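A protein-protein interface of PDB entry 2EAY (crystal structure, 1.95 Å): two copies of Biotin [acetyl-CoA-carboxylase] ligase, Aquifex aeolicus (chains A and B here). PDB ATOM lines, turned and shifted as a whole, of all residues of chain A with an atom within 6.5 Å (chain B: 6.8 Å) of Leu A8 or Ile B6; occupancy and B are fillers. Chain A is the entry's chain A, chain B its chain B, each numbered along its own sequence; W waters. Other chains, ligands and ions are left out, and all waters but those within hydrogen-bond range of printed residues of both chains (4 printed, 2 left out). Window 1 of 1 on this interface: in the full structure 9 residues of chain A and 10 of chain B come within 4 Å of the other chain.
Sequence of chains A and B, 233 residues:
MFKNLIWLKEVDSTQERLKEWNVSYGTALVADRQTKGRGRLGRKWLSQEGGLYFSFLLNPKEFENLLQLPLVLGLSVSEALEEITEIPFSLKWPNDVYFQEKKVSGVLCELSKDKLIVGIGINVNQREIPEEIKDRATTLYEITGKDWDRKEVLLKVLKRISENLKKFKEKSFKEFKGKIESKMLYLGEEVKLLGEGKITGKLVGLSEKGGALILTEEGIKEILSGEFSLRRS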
ATOM      1  N   ILE A   6     -25.192 -25.555 -21.168  1.00  0.00           N
ATOM      2  CA  ILE A   6     -23.838 -25.395 -20.662  1.00  0.00           C
ATOM      3  C   ILE A   6     -23.008 -26.089 -21.747  1.00  0.00           C
ATOM      4  O   ILE A   6     -22.974 -27.316 -21.817  1.00  0.00           O
ATOM      5  CB  ILE A   6     -23.648 -26.109 -19.310  1.00  0.00           C
ATOM      6  CG1 ILE A   6     -24.559 -25.474 -18.256  1.00  0.00           C
ATOM      7  CG2 ILE A   6     -22.200 -26.012 -18.878  1.00  0.00           C
ATOM      8  CD1 ILE A   6     -24.524 -26.179 -16.892  1.00  0.00           C
ATOM      9  N   TRP A   7     -22.364 -25.301 -22.606  1.00  0.00           N
ATOM     10  CA  TRP A   7     -21.584 -25.854 -23.718  1.00  0.00           C
ATOM     11  C   TRP A   7     -20.094 -25.990 -23.441  1.00  0.00           C
ATOM     12  O   TRP A   7     -19.394 -25.007 -23.157  1.00  0.00           O
ATOM     13  CB  TRP A   7     -21.790 -25.007 -24.977  1.00  0.00           C
ATOM     14  CG  TRP A   7     -21.658 -25.801 -26.242  1.00  0.00           C
ATOM     15  CD1 TRP A   7     -20.556 -26.478 -26.677  1.00  0.00           C
ATOM     16  CD2 TRP A   7     -22.676 -26.019 -27.226  1.00  0.00           C
ATOM     17  NE1 TRP A   7     -20.827 -27.113 -27.866  1.00  0.00           N
ATOM     18  CE2 TRP A   7     -22.125 -26.857 -28.220  1.00  0.00           C
ATOM     19  CE3 TRP A   7     -24.009 -25.612 -27.349  1.00  0.00           C
ATOM     20  CZ2 TRP A   7     -22.852 -27.269 -29.342  1.00  0.00           C
ATOM     21  CZ3 TRP A   7     -24.734 -26.024 -28.463  1.00  0.00           C
ATOM     22  CH2 TRP A   7     -24.157 -26.854 -29.438  1.00  0.00           C
ATOM     23  N   LEU A   8     -19.620 -27.222 -23.553  1.00  0.00           N
ATOM     24  CA  LEU A   8     -18.227 -27.562 -23.316  1.00  0.00           C
ATOM     25  C   LEU A   8     -17.490 -27.867 -24.624  1.00  0.00           C
ATOM     26  O   LEU A   8     -18.005 -28.613 -25.468  1.00  0.00           O
ATOM     27  CB  LEU A   8     -18.163 -28.799 -22.420  1.00  0.00           C
ATOM     28  CG  LEU A   8     -18.694 -28.670 -20.990  1.00  0.00           C
ATOM     29  CD1 LEU A   8     -19.393 -29.961 -20.571  1.00  0.00           C
ATOM     30  CD2 LEU A   8     -17.537 -28.361 -20.060  1.00  0.00           C
ATOM     31  N   LYS A   9     -16.296 -27.289 -24.789  1.00  0.00           N
ATOM     32  CA  LYS A   9     -15.470 -27.546 -25.974  1.00  0.00           C
ATOM     33  C   LYS A   9     -14.963 -28.970 -25.837  1.00  0.00           C
ATOM     34  O   LYS A   9     -14.861 -29.705 -26.813  1.00  0.00           O
ATOM     35  CB  LYS A   9     -14.286 -26.583 -26.053  1.00  0.00           C
ATOM     36  CG  LYS A   9     -14.609 -25.307 -26.814  1.00  0.00           C
ATOM     37  CD  LYS A   9     -13.528 -24.238 -26.619  1.00  0.00           C
ATOM     38  CE  LYS A   9     -12.145 -24.789 -26.993  1.00  0.00           C
ATOM     39  NZ  LYS A   9     -11.999 -25.129 -28.426  1.00  0.00           N
ATOM     40  N   GLU A  10     -14.644 -29.364 -24.610  1.00  0.00           N
ATOM     41  CA  GLU A  10     -14.198 -30.729 -24.359  1.00  0.00           C
ATOM     42  C   GLU A  10     -14.423 -31.067 -22.891  1.00  0.00           C
ATOM     43  O   GLU A  10     -14.306 -30.205 -22.016  1.00  0.00           O
ATOM     44  CB  GLU A  10     -12.722 -30.918 -24.743  1.00  0.00           C
ATOM     45  CG  GLU A  10     -11.699 -30.354 -23.773  1.00  0.00           C
ATOM     46  CD  GLU A  10     -10.284 -30.822 -24.102  1.00  0.00           C
ATOM     47  OE1 GLU A  10      -9.685 -30.316 -25.080  1.00  0.00           O
ATOM     48  OE2 GLU A  10      -9.778 -31.717 -23.387  1.00  0.00           O
ATOM     49  N   VAL A  11     -14.768 -32.321 -22.631  1.00  0.00           N
ATOM     50  CA  VAL A  11     -15.037 -32.791 -21.278  1.00  0.00           C
ATOM     51  C   VAL A  11     -14.913 -34.308 -21.317  1.00  0.00           C
ATOM     52  O   VAL A  11     -15.034 -34.913 -22.383  1.00  0.00           O
ATOM     53  CB  VAL A  11     -16.467 -32.404 -20.828  1.00  0.00           C
ATOM     54  CG1 VAL A  11     -17.497 -33.255 -21.567  1.00  0.00           C
ATOM     55  CG2 VAL A  11     -16.614 -32.576 -19.321  1.00  0.00           C
ATOM     56  N   ASP A  12     -14.669 -34.925 -20.165  1.00  0.00           N
ATOM     57  CA  ASP A  12     -14.518 -36.366 -20.124  1.00  0.00           C
ATOM     58  C   ASP A  12     -15.781 -37.084 -20.572  1.00  0.00           C
ATOM     59  O   ASP A  12     -15.733 -37.920 -21.474  1.00  0.00           O
ATOM     60  CB  ASP A  12     -14.087 -36.835 -18.718  1.00  0.00           C
ATOM     61  CG  ASP A  12     -14.952 -36.270 -17.595  1.00  0.00           C
ATOM     62  OD1 ASP A  12     -15.889 -35.500 -17.866  1.00  0.00           O
ATOM     63  OD2 ASP A  12     -14.681 -36.603 -16.420  1.00  0.00           O
ATOM     64  N   SER A  13     -16.913 -36.718 -19.976  1.00  0.00           N
ATOM     65  CA  SER A  13     -18.190 -37.340 -20.300  1.00  0.00           C
ATOM     66  C   SER A  13     -19.340 -36.501 -19.761  1.00  0.00           C
ATOM     67  O   SER A  13     -19.332 -36.115 -18.597  1.00  0.00           O
ATOM     68  CB  SER A  13     -18.249 -38.737 -19.678  1.00  0.00           C
ATOM     69  OG  SER A  13     -19.583 -39.200 -19.593  1.00  0.00           O
ATOM     70  N   THR A  14     -20.336 -36.232 -20.597  1.00  0.00           N
ATOM     71  CA  THR A  14     -21.472 -35.443 -20.148  1.00  0.00           C
ATOM     72  C   THR A  14     -22.323 -36.226 -19.144  1.00  0.00           C
ATOM     73  O   THR A  14     -22.839 -35.647 -18.187  1.00  0.00           O
ATOM     74  CB  THR A  14     -22.342 -34.985 -21.329  1.00  0.00           C
ATOM     75  OG1 THR A  14     -22.860 -36.122 -22.020  1.00  0.00           O
ATOM     76  CG2 THR A  14     -21.513 -34.140 -22.292  1.00  0.00           C
ATOM     77  N   ARG A  17     -20.448 -36.039 -15.696  1.00  0.00           N
ATOM     78  CA  ARG A  17     -20.517 -34.745 -15.031  1.00  0.00           C
ATOM     79  C   ARG A  17     -21.893 -34.477 -14.413  1.00  0.00           C
ATOM     80  O   ARG A  17     -22.027 -33.815 -13.395  1.00  0.00           O
ATOM     81  CB  ARG A  17     -20.168 -33.652 -16.038  1.00  0.00           C
ATOM     82  CG  ARG A  17     -18.688 -33.665 -16.421  1.00  0.00           C
ATOM     83  CD  ARG A  17     -17.738 -33.735 -15.215  1.00  0.00           C
ATOM     84  NE  ARG A  17     -16.348 -33.755 -15.681  1.00  0.00           N
ATOM     85  CZ  ARG A  17     -15.349 -33.895 -14.778  1.00  0.00           C
ATOM     86  NH1 ARG A  17     -15.619 -34.021 -13.488  1.00  0.00           N
ATOM     87  NH2 ARG A  17     -14.086 -33.903 -15.203  1.00  0.00           N
ATOM     88  N   GLU A  20     -21.981 -35.966 -11.178  1.00  0.00           N
ATOM     89  CA  GLU A  20     -21.150 -35.276 -10.182  1.00  0.00           C
ATOM     90  C   GLU A  20     -21.677 -33.883  -9.814  1.00  0.00           C
ATOM     91  O   GLU A  20     -21.635 -33.472  -8.664  1.00  0.00           O
ATOM     92  CB  GLU A  20     -19.733 -35.120 -10.745  1.00  0.00           C
ATOM     93  CG  GLU A  20     -18.974 -36.436 -10.874  1.00  0.00           C
ATOM     94  CD  GLU A  20     -17.668 -36.179 -11.593  1.00  0.00           C
ATOM     95  OE1 GLU A  20     -17.530 -35.139 -12.209  1.00  0.00           O
ATOM     96  OE2 GLU A  20     -16.805 -37.047 -11.547  1.00  0.00           O
ATOM     97  N   TRP A  21     -22.105 -33.103 -10.800  1.00  0.00           N
ATOM     98  CA  TRP A  21     -22.558 -31.739 -10.552  1.00  0.00           C
ATOM     99  C   TRP A  21     -24.066 -31.639 -10.415  1.00  0.00           C
ATOM    100  O   TRP A  21     -24.799 -32.366 -11.086  1.00  0.00           O
ATOM    101  CB  TRP A  21     -22.118 -30.829 -11.700  1.00  0.00           C
ATOM    102  CG  TRP A  21     -20.657 -30.889 -11.993  1.00  0.00           C
ATOM    103  CD1 TRP A  21     -19.656 -31.214 -11.118  1.00  0.00           C
ATOM    104  CD2 TRP A  21     -20.018 -30.567 -13.231  1.00  0.00           C
ATOM    105  NE1 TRP A  21     -18.434 -31.110 -11.736  1.00  0.00           N
ATOM    106  CE2 TRP A  21     -18.626 -30.711 -13.035  1.00  0.00           C
ATOM    107  CE3 TRP A  21     -20.482 -30.160 -14.487  1.00  0.00           C
ATOM    108  CZ2 TRP A  21     -17.695 -30.475 -14.049  1.00  0.00           C
ATOM    109  CZ3 TRP A  21     -19.553 -29.923 -15.499  1.00  0.00           C
ATOM    110  CH2 TRP A  21     -18.177 -30.078 -15.270  1.00  0.00           C
ATOM    111  N   LEU A  29     -26.276 -30.401 -20.697  1.00  0.00           N
ATOM    112  CA  LEU A  29     -24.833 -30.272 -20.635  1.00  0.00           C
ATOM    113  C   LEU A  29     -24.374 -30.780 -21.996  1.00  0.00           C
ATOM    114  O   LEU A  29     -24.490 -31.976 -22.283  1.00  0.00           O
ATOM    115  CB  LEU A  29     -24.257 -31.153 -19.534  1.00  0.00           C
ATOM    116  CG  LEU A  29     -22.758 -30.956 -19.309  1.00  0.00           C
ATOM    117  CD1 LEU A  29     -22.521 -29.560 -18.766  1.00  0.00           C
ATOM    118  CD2 LEU A  29     -22.229 -31.984 -18.332  1.00  0.00           C
ATOM    119  N   VAL A  30     -23.852 -29.873 -22.822  1.00  0.00           N
ATOM    120  CA  VAL A  30     -23.419 -30.214 -24.175  1.00  0.00           C
ATOM    121  C   VAL A  30     -21.905 -30.225 -24.312  1.00  0.00           C
ATOM    122  O   VAL A  30     -21.217 -29.424 -23.693  1.00  0.00           O
ATOM    123  CB  VAL A  30     -23.999 -29.204 -25.194  1.00  0.00           C
ATOM    124  CG1 VAL A  30     -23.703 -29.657 -26.617  1.00  0.00           C
ATOM    125  CG2 VAL A  30     -25.492 -29.051 -24.983  1.00  0.00           C
ATOM    126  N   ALA A  31     -21.390 -31.138 -25.132  1.00  0.00           N
ATOM    127  CA  ALA A  31     -19.949 -31.223 -25.353  1.00  0.00           C
ATOM    128  C   ALA A  31     -19.628 -31.439 -26.833  1.00  0.00           C
ATOM    129  O   ALA A  31     -20.236 -32.244 -27.523  1.00  0.00           O
ATOM    130  CB  ALA A  31     -19.402 -32.389 -24.530  1.00  0.00           C
ATOM    131  N   ASP A  32     -18.659 -30.639 -27.334  1.00  0.00           N
ATOM    132  CA  ASP A  32     -18.235 -30.800 -28.717  1.00  0.00           C
ATOM    133  C   ASP A  32     -17.541 -32.143 -28.922  1.00  0.00           C
ATOM    134  O   ASP A  32     -17.527 -32.730 -29.999  1.00  0.00           O
ATOM    135  CB  ASP A  32     -17.248 -29.685 -29.056  1.00  0.00           C
ATOM    136  CG  ASP A  32     -17.969 -28.348 -29.221  1.00  0.00           C
ATOM    137  OD1 ASP A  32     -19.155 -28.367 -29.537  1.00  0.00           O
ATOM    138  OD2 ASP A  32     -17.331 -27.318 -29.056  1.00  0.00           O
ATOM    139  N   ARG A  33     -16.886 -32.597 -27.845  1.00  0.00           N
ATOM    140  CA  ARG A  33     -16.192 -33.870 -27.893  1.00  0.00           C
ATOM    141  C   ARG A  33     -15.992 -34.411 -26.477  1.00  0.00           C
ATOM    142  O   ARG A  33     -15.872 -33.666 -25.516  1.00  0.00           O
ATOM    143  CB  ARG A  33     -14.833 -33.647 -28.564  1.00  0.00           C
ATOM    144  CG  ARG A  33     -14.161 -34.951 -29.004  1.00  0.00           C
ATOM    145  CD  ARG A  33     -12.918 -34.726 -29.882  1.00  0.00           C
ATOM    146  NE  ARG A  33     -11.923 -33.902 -29.196  1.00  0.00           N
ATOM    147  CZ  ARG A  33     -11.169 -34.477 -28.228  1.00  0.00           C
ATOM    148  NH1 ARG A  33     -11.348 -35.747 -27.907  1.00  0.00           N
ATOM    149  NH2 ARG A  33     -10.234 -33.757 -27.599  1.00  0.00           N
ATOM    150  N   ASN B   4      -7.003 -34.112 -16.341  1.00  0.00           N
ATOM    151  CA  ASN B   4      -8.395 -33.894 -16.698  1.00  0.00           C
ATOM    152  C   ASN B   4      -8.671 -32.426 -17.016  1.00  0.00           C
ATOM    153  O   ASN B   4      -8.286 -31.529 -16.262  1.00  0.00           O
ATOM    154  CB  ASN B   4      -9.303 -34.355 -15.553  1.00  0.00           C
ATOM    155  CG  ASN B   4     -10.710 -34.683 -16.018  1.00  0.00           C
ATOM    156  OD1 ASN B   4     -10.990 -34.699 -17.217  1.00  0.00           O
ATOM    157  ND2 ASN B   4     -11.607 -34.935 -15.069  1.00  0.00           N
ATOM    158  N   LEU B   5      -9.326 -32.186 -18.146  1.00  0.00           N
ATOM    159  CA  LEU B   5      -9.665 -30.829 -18.552  1.00  0.00           C
ATOM    160  C   LEU B   5     -11.165 -30.680 -18.766  1.00  0.00           C
ATOM    161  O   LEU B   5     -11.808 -31.542 -19.368  1.00  0.00           O
ATOM    162  CB  LEU B   5      -8.948 -30.450 -19.854  1.00  0.00           C
ATOM    163  CG  LEU B   5      -7.427 -30.299 -19.881  1.00  0.00           C
ATOM    164  CD1 LEU B   5      -6.991 -29.968 -21.304  1.00  0.00           C
ATOM    165  CD2 LEU B   5      -6.983 -29.204 -18.929  1.00  0.00           C
ATOM    166  N   ILE B   6     -11.715 -29.590 -18.244  1.00  0.00           N
ATOM    167  CA  ILE B   6     -13.124 -29.265 -18.401  1.00  0.00           C
ATOM    168  C   ILE B   6     -13.054 -27.899 -19.057  1.00  0.00           C
ATOM    169  O   ILE B   6     -12.736 -26.910 -18.396  1.00  0.00           O
ATOM    170  CB  ILE B   6     -13.846 -29.108 -17.056  1.00  0.00           C
ATOM    171  CG1 ILE B   6     -13.743 -30.401 -16.243  1.00  0.00           C
ATOM    172  CG2 ILE B   6     -15.304 -28.737 -17.305  1.00  0.00           C
ATOM    173  CD1 ILE B   6     -14.398 -30.313 -14.875  1.00  0.00           C
ATOM    174  N   TRP B   7     -13.337 -27.842 -20.353  1.00  0.00           N
ATOM    175  CA  TRP B   7     -13.245 -26.584 -21.080  1.00  0.00           C
ATOM    176  C   TRP B   7     -14.613 -26.068 -21.503  1.00  0.00           C
ATOM    177  O   TRP B   7     -15.255 -26.646 -22.379  1.00  0.00           O
ATOM    178  CB  TRP B   7     -12.349 -26.777 -22.311  1.00  0.00           C
ATOM    179  CG  TRP B   7     -11.732 -25.515 -22.858  1.00  0.00           C
ATOM    180  CD1 TRP B   7     -12.370 -24.340 -23.131  1.00  0.00           C
ATOM    181  CD2 TRP B   7     -10.363 -25.326 -23.253  1.00  0.00           C
ATOM    182  NE1 TRP B   7     -11.488 -23.432 -23.674  1.00  0.00           N
ATOM    183  CE2 TRP B   7     -10.249 -24.014 -23.761  1.00  0.00           C
ATOM    184  CE3 TRP B   7      -9.226 -26.143 -23.231  1.00  0.00           C
ATOM    185  CZ2 TRP B   7      -9.042 -23.493 -24.242  1.00  0.00           C
ATOM    186  CZ3 TRP B   7      -8.017 -25.625 -23.713  1.00  0.00           C
ATOM    187  CH2 TRP B   7      -7.939 -24.311 -24.211  1.00  0.00           C
ATOM    188  N   LEU B   8     -15.048 -24.981 -20.867  1.00  0.00           N
ATOM    189  CA  LEU B   8     -16.330 -24.349 -21.173  1.00  0.00           C
ATOM    190  C   LEU B   8     -16.126 -23.206 -22.165  1.00  0.00           C
ATOM    191  O   LEU B   8     -15.073 -22.563 -22.189  1.00  0.00           O
ATOM    192  CB  LEU B   8     -16.968 -23.761 -19.913  1.00  0.00           C
ATOM    193  CG  LEU B   8     -17.465 -24.572 -18.708  1.00  0.00           C
ATOM    194  CD1 LEU B   8     -18.635 -25.437 -19.122  1.00  0.00           C
ATOM    195  CD2 LEU B   8     -16.335 -25.385 -18.115  1.00  0.00           C
ATOM    196  N   LYS B   9     -17.144 -22.941 -22.972  1.00  0.00           N
ATOM    197  CA  LYS B   9     -17.080 -21.855 -23.935  1.00  0.00           C
ATOM    198  C   LYS B   9     -17.261 -20.530 -23.195  1.00  0.00           C
ATOM    199  O   LYS B   9     -16.642 -19.530 -23.539  1.00  0.00           O
ATOM    200  CB  LYS B   9     -18.176 -22.022 -24.990  1.00  0.00           C
ATOM    201  CG  LYS B   9     -18.002 -23.258 -25.856  1.00  0.00           C
ATOM    202  CD  LYS B   9     -18.434 -23.029 -27.296  1.00  0.00           C
ATOM    203  CE  LYS B   9     -19.897 -22.618 -27.416  1.00  0.00           C
ATOM    204  NZ  LYS B   9     -20.080 -21.138 -27.499  1.00  0.00           N
ATOM    205  N   LEU B  18     -15.782 -23.429  -9.961  1.00  0.00           N
ATOM    206  CA  LEU B  18     -15.120 -24.395  -9.094  1.00  0.00           C
ATOM    207  C   LEU B  18     -15.645 -24.319  -7.656  1.00  0.00           C
ATOM    208  O   LEU B  18     -15.397 -25.216  -6.847  1.00  0.00           O
ATOM    209  CB  LEU B  18     -13.610 -24.174  -9.129  1.00  0.00           C
ATOM    210  CG  LEU B  18     -12.785 -25.302  -9.757  1.00  0.00           C
ATOM    211  CD1 LEU B  18     -13.471 -25.828 -11.010  1.00  0.00           C
ATOM    212  CD2 LEU B  18     -11.388 -24.807 -10.073  1.00  0.00           C
ATOM    213  N   TRP B  21     -19.309 -26.462  -8.696  1.00  0.00           N
ATOM    214  CA  TRP B  21     -19.105 -27.813  -9.202  1.00  0.00           C
ATOM    215  C   TRP B  21     -17.889 -28.473  -8.588  1.00  0.00           C
ATOM    216  O   TRP B  21     -16.765 -28.000  -8.760  1.00  0.00           O
ATOM    217  CB  TRP B  21     -18.934 -27.813 -10.727  1.00  0.00           C
ATOM    218  CG  TRP B  21     -20.097 -27.272 -11.491  1.00  0.00           C
ATOM    219  CD1 TRP B  21     -21.394 -27.198 -11.073  1.00  0.00           C
ATOM    220  CD2 TRP B  21     -20.076 -26.764 -12.832  1.00  0.00           C
ATOM    221  NE1 TRP B  21     -22.182 -26.674 -12.070  1.00  0.00           N
ATOM    222  CE2 TRP B  21     -21.401 -26.398 -13.157  1.00  0.00           C
ATOM    223  CE3 TRP B  21     -19.066 -26.583 -13.787  1.00  0.00           C
ATOM    224  CZ2 TRP B  21     -21.744 -25.860 -14.407  1.00  0.00           C
ATOM    225  CZ3 TRP B  21     -19.407 -26.049 -15.028  1.00  0.00           C
ATOM    226  CH2 TRP B  21     -20.740 -25.692 -15.324  1.00  0.00           C
ATOM    227  N   ASN B  22     -18.109 -29.577  -7.886  1.00  0.00           N
ATOM    228  CA  ASN B  22     -17.004 -30.286  -7.270  1.00  0.00           C
ATOM    229  C   ASN B  22     -16.092 -30.863  -8.341  1.00  0.00           C
ATOM    230  O   ASN B  22     -16.548 -31.472  -9.315  1.00  0.00           O
ATOM    231  CB  ASN B  22     -17.519 -31.392  -6.352  1.00  0.00           C
ATOM    232  CG  ASN B  22     -18.331 -30.846  -5.197  1.00  0.00           C
ATOM    233  OD1 ASN B  22     -19.346 -31.427  -4.812  1.00  0.00           O
ATOM    234  ND2 ASN B  22     -17.892 -29.724  -4.639  1.00  0.00           N
ATOM    235  N   VAL B  23     -14.797 -30.656  -8.150  1.00  0.00           N
ATOM    236  CA  VAL B  23     -13.794 -31.130  -9.081  1.00  0.00           C
ATOM    237  C   VAL B  23     -12.673 -31.792  -8.293  1.00  0.00           C
ATOM    238  O   VAL B  23     -12.442 -31.453  -7.135  1.00  0.00           O
ATOM    239  CB  VAL B  23     -13.225 -29.949  -9.892  1.00  0.00           C
ATOM    240  CG1 VAL B  23     -12.121 -30.421 -10.791  1.00  0.00           C
ATOM    241  CG2 VAL B  23     -14.334 -29.300 -10.709  1.00  0.00           C
ATOM    242  N   THR B  27      -7.469 -31.457 -12.074  1.00  0.00           N
ATOM    243  CA  THR B  27      -8.438 -31.053 -13.080  1.00  0.00           C
ATOM    244  C   THR B  27      -8.465 -29.530 -13.235  1.00  0.00           C
ATOM    245  O   THR B  27      -8.603 -28.797 -12.258  1.00  0.00           O
ATOM    246  CB  THR B  27      -9.856 -31.523 -12.703  1.00  0.00           C
ATOM    247  OG1 THR B  27      -9.901 -32.955 -12.668  1.00  0.00           O
ATOM    248  CG2 THR B  27     -10.869 -31.010 -13.711  1.00  0.00           C
ATOM    249  N   ALA B  28      -8.328 -29.057 -14.467  1.00  0.00           N
ATOM    250  CA  ALA B  28      -8.367 -27.624 -14.728  1.00  0.00           C
ATOM    251  C   ALA B  28      -9.703 -27.291 -15.363  1.00  0.00           C
ATOM    252  O   ALA B  28     -10.149 -27.985 -16.281  1.00  0.00           O
ATOM    253  CB  ALA B  28      -7.234 -27.219 -15.660  1.00  0.00           C
ATOM    254  N   LEU B  29     -10.356 -26.248 -14.859  1.00  0.00           N
ATOM    255  CA  LEU B  29     -11.631 -25.826 -15.418  1.00  0.00           C
ATOM    256  C   LEU B  29     -11.309 -24.583 -16.227  1.00  0.00           C
ATOM    257  O   LEU B  29     -10.962 -23.533 -15.677  1.00  0.00           O
ATOM    258  CB  LEU B  29     -12.644 -25.519 -14.317  1.00  0.00           C
ATOM    259  CG  LEU B  29     -14.054 -25.227 -14.847  1.00  0.00           C
ATOM    260  CD1 LEU B  29     -15.093 -25.806 -13.906  1.00  0.00           C
ATOM    261  CD2 LEU B  29     -14.236 -23.724 -15.016  1.00  0.00           C
ATOM    262  N   VAL B  30     -11.422 -24.730 -17.539  1.00  0.00           N
ATOM    263  CA  VAL B  30     -11.099 -23.675 -18.482  1.00  0.00           C
ATOM    264  C   VAL B  30     -12.344 -23.052 -19.088  1.00  0.00           C
ATOM    265  O   VAL B  30     -13.395 -23.691 -19.178  1.00  0.00           O
ATOM    266  CB  VAL B  30     -10.214 -24.237 -19.633  1.00  0.00           C
ATOM    267  CG1 VAL B  30      -9.551 -23.105 -20.397  1.00  0.00           C
ATOM    268  CG2 VAL B  30      -9.200 -25.220 -19.084  1.00  0.00           C
ATOM    269  N   ALA B  31     -12.216 -21.791 -19.488  1.00  0.00           N
ATOM    270  CA  ALA B  31     -13.292 -21.066 -20.140  1.00  0.00           C
ATOM    271  C   ALA B  31     -12.702 -20.118 -21.178  1.00  0.00           C
ATOM    272  O   ALA B  31     -11.656 -19.522 -20.986  1.00  0.00           O
ATOM    273  CB  ALA B  31     -14.052 -20.275 -19.083  1.00  0.00           C
HETATM  274  O   HOH W   1     -20.781 -30.514  -7.409  1.00  0.00           O
HETATM  275  O   HOH W   2     -12.850 -33.753 -12.052  1.00  0.00           O
HETATM  276  O   HOH W   3     -11.468 -33.163 -21.645  1.00  0.00           O
HETATM  277  O   HOH W   4     -12.689 -37.827 -15.662  1.00  0.00           O
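N of Lys B9 lies within hydrogen-bond range of O of Trp A7 (3.1 Å). The backbone carbonyl oxygen of Trp B7 lies within hydrogen-bond range of the backbone NH of Lys A9 (2.7 Å). N of Trp B7 sits at hydrogen-bond distance from O of Glu A10 (3.0 Å). The guanidinium group (NH2) of Arg A17 lies close to the side-chain amide nitrogen (ND2) of Asn B4, 2.7 Å away. The indole nitrogen (NE1) of Trp A21 lies within hydrogen-bond range of the backbone carbonyl oxygen (O) of Asn B22 (3.1 Å).
The backbone carbonyl oxygen of Ile A6 is in hydrogen-bond range of the backbone NH of Val A30, 2.9 Å away. The indole nitrogen (NE1) of Trp A7 lies within hydrogen-bond range of the side-chain carboxylate (OD1) of Asp A32. O of Leu A8 is in hydrogen-bond range of N of Asp A32 (2.8 Å). The side-chain carboxylate of Asp A12 lies within salt-bridge range of the guanidinium group of Arg A17 (2.8 Å). OE1 of Glu A20 is in salt-bridge range of NH1 of Arg A17 (2.6 Å). The backbone carbonyl oxygen (O) of Ala B28 is in hydrogen-bond range of the backbone NH (N) of Ile B6 (3.0 Å).
Ile A6 touches Leu B8 (CG2 to CD1, 3.6 Å). CD1 of Ile A6 touches CZ2 of Trp B21, 3.7 Å away. Trp A7 touches Leu B8. Leu A8 touches Ile B6 (CD2 to CG2, 3.6 Å). O of Trp B7 touches CA of Leu A8 (3.2 Å). CD1 of Leu B8 touches CD2 of Leu A8 (3.3 Å). Glu A10 touches Ile B6. ND2 of Asn B4 touches OD2 of Asp A12 (3.7 Å). Ile B6 touches Arg A17 (CD1 to NH2, 3.6 Å). Trp A21 touches Trp B21 (NE1 to CB, 3.5 Å).
Leu A8 touches just these residues of chain B: Ile B6, Trp B7 and Leu B8. Of chain A, only Leu A8 (3.6 Å), Glu A10 (3.9 Å), Arg A17 (3.6 Å) and Trp A21 (3.4 Å) come within 4 Å of Ile B6. Of the printed residues of chain B, Ile A6 touches Leu B8 (3.6 Å) and Trp B21 (3.7 Å). Printed residues of chain B within 4 Å of Val A11: Leu B5 (3.95 Å). Of the printed residues of chain A, Asn B22 touches Trp A21 (3.1 Å). Printed residues of chain A within 4 Å of Leu B5: Glu A10 (3.8 Å) and Val A11 (3.95 Å). Val B30 touches none of the printed residues of chain A. Leu A29 touches none of the printed residues of chain B. The nearest printed residue of chain B that does not touch Ile A6 is Lys B9 (6.8 Å).
Of the 15 printed residues of chain B, 8 touch a printed residue of chain A. Hydrophobic or aromatic side chains of chain B that line the printed part of chain A: Leu B5, Ile B6, Trp B7, Leu B8 and Trp B21. Of the 17 printed residues of chain A, 9 touch a printed residue of chain B. Printed residues of chain A that touch a printed residue of chain B: Ile A6, Trp A7, Leu A8, Lys A9, Glu A10, Val A11, Asp A12, Arg A17 and Trp A21. Hydrophobic or aromatic side chains of chain A that line the printed part of chain B: Ile A6, Trp A7, Leu A8 and Trp A21.
Ile A6 touches Leu B8, and with the chains exchanged Leu A8 touches Ile B6. Ile A6 touches Trp B21, and with the chains exchanged Trp A21 touches Ile B6. Trp A7 touches Leu B8, and with the chains exchanged Leu A8 touches Trp B7. Leu A8 touches its own counterpart, Leu B8. 8 positions are printed for both chains.
Water W4 lies within hydrogen-bond range of OD2 of Asp A12 (2.5 Å) and ND2 of Asn B4 (3.1 Å). Water W3 bridges the backbone carbonyl oxygen (O) of Leu B5 and the side-chain carboxylate (OE2) of Glu A10. Water W1 lies within hydrogen-bond range of N of Asn B22 (2.9 Å) and O of Glu A20 (3.3 Å). Water W2 lies within hydrogen-bond range of the side-chain hydroxyl (OG1) of Thr B27 (3.1 Å), the guanidinium group (NH1) of Arg A17 (3.1 Å) and the side-chain amide nitrogen (ND2) of Asn B4 (3.5 Å).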
